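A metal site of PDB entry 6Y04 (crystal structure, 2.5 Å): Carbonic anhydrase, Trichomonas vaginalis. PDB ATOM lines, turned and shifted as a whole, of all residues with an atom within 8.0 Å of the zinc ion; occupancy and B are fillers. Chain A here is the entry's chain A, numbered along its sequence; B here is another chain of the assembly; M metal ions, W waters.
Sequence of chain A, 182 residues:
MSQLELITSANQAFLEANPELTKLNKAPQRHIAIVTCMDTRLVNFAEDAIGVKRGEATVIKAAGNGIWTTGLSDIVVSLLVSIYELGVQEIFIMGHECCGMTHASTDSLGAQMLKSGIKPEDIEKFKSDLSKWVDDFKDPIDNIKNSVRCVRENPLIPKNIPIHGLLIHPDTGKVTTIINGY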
ATOM      1  N   THR A  36     -22.373 -19.808 -29.062  1.00  0.00           N
ATOM      2  CA  THR A  36     -21.083 -19.889 -28.391  1.00  0.00           C
ATOM      3  C   THR A  36     -20.180 -18.743 -28.845  1.00  0.00           C
ATOM      4  O   THR A  36     -20.630 -17.846 -29.560  1.00  0.00           O
ATOM      5  CB  THR A  36     -20.495 -21.306 -28.479  1.00  0.00           C
ATOM      6  OG1 THR A  36     -19.502 -21.420 -27.456  1.00  0.00           O
ATOM      7  CG2 THR A  36     -19.906 -21.649 -29.831  1.00  0.00           C
ATOM      8  N   CYS A  37     -18.923 -18.787 -28.397  1.00  0.00           N
ATOM      9  CA  CYS A  37     -17.983 -17.686 -28.597  1.00  0.00           C
ATOM     10  C   CYS A  37     -17.202 -17.883 -29.898  1.00  0.00           C
ATOM     11  O   CYS A  37     -17.081 -18.991 -30.410  1.00  0.00           O
ATOM     12  CB  CYS A  37     -17.029 -17.566 -27.427  1.00  0.00           C
ATOM     13  SG  CYS A  37     -15.965 -16.098 -27.579  1.00  0.00           S
ATOM     14  N   MET A  38     -16.641 -16.783 -30.399  1.00  0.00           N
ATOM     15  CA  MET A  38     -15.879 -16.822 -31.641  1.00  0.00           C
ATOM     16  C   MET A  38     -14.464 -17.358 -31.387  1.00  0.00           C
ATOM     17  O   MET A  38     -13.688 -17.497 -32.323  1.00  0.00           O
ATOM     18  CB  MET A  38     -15.792 -15.427 -32.261  1.00  0.00           C
ATOM     19  CG  MET A  38     -14.908 -14.501 -31.471  1.00  0.00           C
ATOM     20  SD  MET A  38     -14.779 -12.854 -32.189  1.00  0.00           S
ATOM     21  CE  MET A  38     -13.454 -12.162 -31.203  1.00  0.00           C
ATOM     22  N   ASP A  39     -14.147 -17.654 -30.118  1.00  0.00           N
ATOM     23  CA  ASP A  39     -12.802 -17.971 -29.655  1.00  0.00           C
ATOM     24  C   ASP A  39     -12.141 -18.988 -30.594  1.00  0.00           C
ATOM     25  O   ASP A  39     -12.732 -20.008 -30.957  1.00  0.00           O
ATOM     26  CB  ASP A  39     -12.791 -18.421 -28.191  1.00  0.00           C
ATOM     27  CG  ASP A  39     -11.407 -18.468 -27.554  1.00  0.00           C
ATOM     28  OD1 ASP A  39     -10.620 -19.358 -27.923  1.00  0.00           O
ATOM     29  OD2 ASP A  39     -11.129 -17.617 -26.690  1.00  0.00           O
ATOM     30  N   THR A  40     -10.877 -18.695 -30.951  1.00  0.00           N
ATOM     31  CA  THR A  40     -10.123 -19.517 -31.889  1.00  0.00           C
ATOM     32  C   THR A  40     -10.032 -20.976 -31.429  1.00  0.00           C
ATOM     33  O   THR A  40      -9.925 -21.874 -32.264  1.00  0.00           O
ATOM     34  CB  THR A  40      -8.721 -18.931 -32.141  1.00  0.00           C
ATOM     35  OG1 THR A  40      -8.243 -19.574 -33.324  1.00  0.00           O
ATOM     36  CG2 THR A  40      -7.749 -19.142 -31.002  1.00  0.00           C
ATOM     37  N   ARG A  41     -10.101 -21.203 -30.115  1.00  0.00           N
ATOM     38  CA  ARG A  41      -9.838 -22.501 -29.517  1.00  0.00           C
ATOM     39  C   ARG A  41     -11.062 -23.423 -29.622  1.00  0.00           C
ATOM     40  O   ARG A  41     -10.941 -24.627 -29.408  1.00  0.00           O
ATOM     41  CB  ARG A  41      -9.405 -22.332 -28.056  1.00  0.00           C
ATOM     42  CG  ARG A  41      -7.993 -21.780 -27.903  1.00  0.00           C
ATOM     43  CD  ARG A  41      -7.651 -21.360 -26.486  1.00  0.00           C
ATOM     44  NE  ARG A  41      -8.496 -20.251 -26.083  1.00  0.00           N
ATOM     45  CZ  ARG A  41      -8.411 -19.614 -24.927  1.00  0.00           C
ATOM     46  NH1 ARG A  41      -7.496 -19.965 -24.036  1.00  0.00           N
ATOM     47  NH2 ARG A  41      -9.249 -18.620 -24.662  1.00  0.00           N
ATOM     48  N   LEU A  42     -12.232 -22.843 -29.931  1.00  0.00           N
ATOM     49  CA  LEU A  42     -13.479 -23.597 -29.985  1.00  0.00           C
ATOM     50  C   LEU A  42     -13.745 -24.083 -31.409  1.00  0.00           C
ATOM     51  O   LEU A  42     -14.584 -24.966 -31.599  1.00  0.00           O
ATOM     52  CB  LEU A  42     -14.628 -22.758 -29.448  1.00  0.00           C
ATOM     53  CG  LEU A  42     -14.460 -22.249 -28.006  1.00  0.00           C
ATOM     54  CD1 LEU A  42     -15.645 -21.371 -27.602  1.00  0.00           C
ATOM     55  CD2 LEU A  42     -14.284 -23.400 -27.040  1.00  0.00           C
ATOM     56  N   ALA A  62     -20.499 -15.269 -31.538  1.00  0.00           N
ATOM     57  CA  ALA A  62     -20.046 -13.898 -31.413  1.00  0.00           C
ATOM     58  C   ALA A  62     -19.078 -13.807 -30.237  1.00  0.00           C
ATOM     59  O   ALA A  62     -19.112 -14.651 -29.350  1.00  0.00           O
ATOM     60  CB  ALA A  62     -21.229 -12.971 -31.226  1.00  0.00           C
ATOM     61  N   ALA A  63     -18.257 -12.756 -30.229  1.00  0.00           N
ATOM     62  CA  ALA A  63     -17.341 -12.497 -29.125  1.00  0.00           C
ATOM     63  C   ALA A  63     -18.125 -12.446 -27.809  1.00  0.00           C
ATOM     64  O   ALA A  63     -18.878 -11.509 -27.579  1.00  0.00           O
ATOM     65  CB  ALA A  63     -16.591 -11.220 -29.375  1.00  0.00           C
ATOM     66  N   GLY A  64     -17.948 -13.478 -26.969  1.00  0.00           N
ATOM     67  CA  GLY A  64     -18.523 -13.486 -25.634  1.00  0.00           C
ATOM     68  C   GLY A  64     -19.946 -14.067 -25.589  1.00  0.00           C
ATOM     69  O   GLY A  64     -20.542 -14.123 -24.512  1.00  0.00           O
ATOM     70  N   ASN A  65     -20.462 -14.488 -26.743  1.00  0.00           N
ATOM     71  CA  ASN A  65     -21.719 -15.228 -26.852  1.00  0.00           C
ATOM     72  C   ASN A  65     -22.815 -14.613 -25.972  1.00  0.00           C
ATOM     73  O   ASN A  65     -23.525 -15.321 -25.264  1.00  0.00           O
ATOM     74  CB  ASN A  65     -21.535 -16.711 -26.513  1.00  0.00           C
ATOM     75  CG  ASN A  65     -20.847 -16.939 -25.179  1.00  0.00           C
ATOM     76  OD1 ASN A  65     -19.622 -16.961 -25.114  1.00  0.00           O
ATOM     77  ND2 ASN A  65     -21.620 -17.088 -24.119  1.00  0.00           N
ATOM     78  N   MET A  94     -23.633 -21.386 -24.609  1.00  0.00           N
ATOM     79  CA  MET A  94     -22.424 -22.011 -24.091  1.00  0.00           C
ATOM     80  C   MET A  94     -21.272 -21.010 -24.073  1.00  0.00           C
ATOM     81  O   MET A  94     -20.673 -20.709 -25.119  1.00  0.00           O
ATOM     82  CB  MET A  94     -22.051 -23.233 -24.933  1.00  0.00           C
ATOM     83  CG  MET A  94     -20.782 -23.901 -24.464  1.00  0.00           C
ATOM     84  SD  MET A  94     -20.565 -25.541 -25.140  1.00  0.00           S
ATOM     85  CE  MET A  94     -20.252 -25.142 -26.854  1.00  0.00           C
ATOM     86  N   GLY A  95     -20.977 -20.508 -22.867  1.00  0.00           N
ATOM     87  CA  GLY A  95     -19.830 -19.638 -22.629  1.00  0.00           C
ATOM     88  C   GLY A  95     -18.585 -20.444 -22.317  1.00  0.00           C
ATOM     89  O   GLY A  95     -18.626 -21.674 -22.293  1.00  0.00           O
ATOM     90  N   HIS A  96     -17.475 -19.763 -22.069  1.00  0.00           N
ATOM     91  CA  HIS A  96     -16.229 -20.460 -21.797  1.00  0.00           C
ATOM     92  C   HIS A  96     -15.366 -19.671 -20.827  1.00  0.00           C
ATOM     93  O   HIS A  96     -15.435 -18.444 -20.780  1.00  0.00           O
ATOM     94  CB  HIS A  96     -15.490 -20.774 -23.109  1.00  0.00           C
ATOM     95  CG  HIS A  96     -14.924 -19.570 -23.784  1.00  0.00           C
ATOM     96  ND1 HIS A  96     -13.563 -19.300 -23.770  1.00  0.00           N
ATOM     97  CD2 HIS A  96     -15.504 -18.562 -24.473  1.00  0.00           C
ATOM     98  CE1 HIS A  96     -13.340 -18.187 -24.441  1.00  0.00           C
ATOM     99  NE2 HIS A  96     -14.504 -17.706 -24.871  1.00  0.00           N
ATOM    100  N   GLU A  97     -14.551 -20.414 -20.064  1.00  0.00           N
ATOM    101  CA  GLU A  97     -13.572 -19.868 -19.139  1.00  0.00           C
ATOM    102  C   GLU A  97     -12.474 -19.198 -19.947  1.00  0.00           C
ATOM    103  O   GLU A  97     -12.198 -19.608 -21.076  1.00  0.00           O
ATOM    104  CB  GLU A  97     -13.006 -21.006 -18.266  1.00  0.00           C
ATOM    105  CG  GLU A  97     -14.038 -22.067 -17.928  1.00  0.00           C
ATOM    106  CD  GLU A  97     -13.690 -23.073 -16.841  1.00  0.00           C
ATOM    107  OE1 GLU A  97     -12.918 -22.705 -15.917  1.00  0.00           O
ATOM    108  OE2 GLU A  97     -14.188 -24.224 -16.904  1.00  0.00           O
ATOM    109  N   CYS A  98     -11.856 -18.157 -19.378  1.00  0.00           N
ATOM    110  CA  CYS A  98     -10.771 -17.423 -20.001  1.00  0.00           C
ATOM    111  C   CYS A  98     -11.269 -16.699 -21.263  1.00  0.00           C
ATOM    112  O   CYS A  98     -10.554 -16.646 -22.254  1.00  0.00           O
ATOM    113  CB  CYS A  98      -9.596 -18.328 -20.373  1.00  0.00           C
ATOM    114  SG  CYS A  98      -8.962 -19.373 -19.032  1.00  0.00           S
ATOM    115  N   CYS A  99     -12.504 -16.168 -21.210  1.00  0.00           N
ATOM    116  CA  CYS A  99     -13.085 -15.503 -22.364  1.00  0.00           C
ATOM    117  C   CYS A  99     -12.408 -14.149 -22.512  1.00  0.00           C
ATOM    118  O   CYS A  99     -12.095 -13.514 -21.500  1.00  0.00           O
ATOM    119  CB  CYS A  99     -14.599 -15.309 -22.192  1.00  0.00           C
ATOM    120  SG  CYS A  99     -15.430 -14.681 -23.682  1.00  0.00           S
ATOM    121  N   GLY A 100     -12.152 -13.716 -23.756  1.00  0.00           N
ATOM    122  CA  GLY A 100     -11.348 -12.534 -24.031  1.00  0.00           C
ATOM    123  C   GLY A 100     -12.100 -11.226 -23.771  1.00  0.00           C
ATOM    124  O   GLY A 100     -11.544 -10.129 -23.873  1.00  0.00           O
ATOM    125  N   MET A 101     -13.383 -11.383 -23.406  1.00  0.00           N
ATOM    126  CA  MET A 101     -14.345 -10.303 -23.333  1.00  0.00           C
ATOM    127  C   MET A 101     -14.417  -9.789 -21.896  1.00  0.00           C
ATOM    128  O   MET A 101     -14.902  -8.679 -21.667  1.00  0.00           O
ATOM    129  CB  MET A 101     -15.717 -10.814 -23.759  1.00  0.00           C
ATOM    130  CG  MET A 101     -15.878 -10.841 -25.265  1.00  0.00           C
ATOM    131  SD  MET A 101     -15.949  -9.152 -25.938  1.00  0.00           S
ATOM    132  CE  MET A 101     -17.699  -8.786 -25.755  1.00  0.00           C
ATOM    133  N   THR A 102     -13.939 -10.616 -20.967  1.00  0.00           N
ATOM    134  CA  THR A 102     -13.824 -10.271 -19.556  1.00  0.00           C
ATOM    135  C   THR A 102     -12.900  -9.061 -19.390  1.00  0.00           C
ATOM    136  O   THR A 102     -13.321  -8.051 -18.827  1.00  0.00           O
ATOM    137  CB  THR A 102     -13.320 -11.474 -18.729  1.00  0.00           C
ATOM    138  OG1 THR A 102     -13.875 -12.686 -19.235  1.00  0.00           O
ATOM    139  CG2 THR A 102     -13.636 -11.356 -17.258  1.00  0.00           C
ATOM    140  N   PHE A 137     -19.836  -7.236 -19.815  1.00  0.00           N
ATOM    141  CA  PHE A 137     -19.276  -8.577 -19.719  1.00  0.00           C
ATOM    142  C   PHE A 137     -18.329  -8.670 -18.515  1.00  0.00           C
ATOM    143  O   PHE A 137     -17.144  -8.373 -18.620  1.00  0.00           O
ATOM    144  CB  PHE A 137     -18.606  -9.008 -21.029  1.00  0.00           C
ATOM    145  CG  PHE A 137     -18.348 -10.486 -21.154  1.00  0.00           C
ATOM    146  CD1 PHE A 137     -17.399 -11.124 -20.363  1.00  0.00           C
ATOM    147  CD2 PHE A 137     -19.057 -11.255 -22.073  1.00  0.00           C
ATOM    148  CE1 PHE A 137     -17.161 -12.483 -20.475  1.00  0.00           C
ATOM    149  CE2 PHE A 137     -18.812 -12.620 -22.185  1.00  0.00           C
ATOM    150  CZ  PHE A 137     -17.873 -13.238 -21.390  1.00  0.00           C
ATOM    151  N   PRO A 140     -17.621 -14.900 -17.285  1.00  0.00           N
ATOM    152  CA  PRO A 140     -18.254 -15.890 -18.166  1.00  0.00           C
ATOM    153  C   PRO A 140     -19.531 -16.551 -17.629  1.00  0.00           C
ATOM    154  O   PRO A 140     -20.507 -16.678 -18.373  1.00  0.00           O
ATOM    155  CB  PRO A 140     -17.146 -16.929 -18.396  1.00  0.00           C
ATOM    156  CG  PRO A 140     -15.861 -16.148 -18.208  1.00  0.00           C
ATOM    157  CD  PRO A 140     -16.191 -15.154 -17.117  1.00  0.00           C
ATOM    158  N   PRO A 170     -11.840 -23.994 -22.673  1.00  0.00           N
ATOM    159  CA  PRO A 170     -11.272 -23.918 -24.021  1.00  0.00           C
ATOM    160  C   PRO A 170     -10.029 -24.789 -24.257  1.00  0.00           C
ATOM    161  O   PRO A 170      -9.646 -25.004 -25.403  1.00  0.00           O
ATOM    162  CB  PRO A 170     -10.993 -22.421 -24.203  1.00  0.00           C
ATOM    163  CG  PRO A 170     -10.790 -21.889 -22.796  1.00  0.00           C
ATOM    164  CD  PRO A 170     -11.653 -22.754 -21.895  1.00  0.00           C
ATOM    165  N   VAL B  81     -13.119  -6.737 -31.622  1.00  0.00           N
ATOM    166  CA  VAL B  81     -12.398  -7.528 -30.641  1.00  0.00           C
ATOM    167  C   VAL B  81     -11.312  -8.334 -31.356  1.00  0.00           C
ATOM    168  O   VAL B  81     -10.183  -8.408 -30.885  1.00  0.00           O
ATOM    169  CB  VAL B  81     -13.349  -8.415 -29.823  1.00  0.00           C
ATOM    170  CG1 VAL B  81     -12.596  -9.364 -28.897  1.00  0.00           C
ATOM    171  CG2 VAL B  81     -14.361  -7.592 -29.043  1.00  0.00           C
ATOM    172  N   LEU B  86      -7.240  -9.197 -30.383  1.00  0.00           N
ATOM    173  CA  LEU B  86      -6.739 -10.533 -30.675  1.00  0.00           C
ATOM    174  C   LEU B  86      -5.790 -10.591 -31.868  1.00  0.00           C
ATOM    175  O   LEU B  86      -5.368 -11.681 -32.257  1.00  0.00           O
ATOM    176  CB  LEU B  86      -7.921 -11.489 -30.866  1.00  0.00           C
ATOM    177  CG  LEU B  86      -8.695 -11.813 -29.588  1.00  0.00           C
ATOM    178  CD1 LEU B  86     -10.005 -12.524 -29.906  1.00  0.00           C
ATOM    179  CD2 LEU B  86      -7.843 -12.653 -28.645  1.00  0.00           C
HETATM  180 ZN    ZN M   1     -14.739 -15.811 -25.608  1.00  0.00          ZN
HETATM  181  O   HOH W   1     -13.108 -14.863 -26.255  1.00  0.00           O
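The zinc ion is bound by water W1 (2.0 Å), a ring nitrogen (NE2) of His 96 (2.0 Å), the side-chain sulfur of Cys 37 (2.3 Å) and the side-chain sulfur of Cys 99 (2.3 Å).
Water W1 bridges the backbone NH of Gly 100 and the side-chain carboxylate of Asp 39.
N of Asp 39 sits close to SG of Cys 37.
N of Gly 64 sits close to SG of Cys 37 (3.3 Å).
O of Cys 99 is in hydrogen-bond range of OG1 of Thr 102, at 3.0 Å.
Gly 100 touches the zinc ion (N to ZN, 3.8 Å).
Four residues have an atom within 4 Å of the zinc ion: Cys 37, His 96, Cys 99 and Gly 100.
Along chain A the residues within 4 Å of the zinc ion span positions 37 to 100.
The nearest printed residue that does not touch the zinc ion is Asp 39 (4.2 Å).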
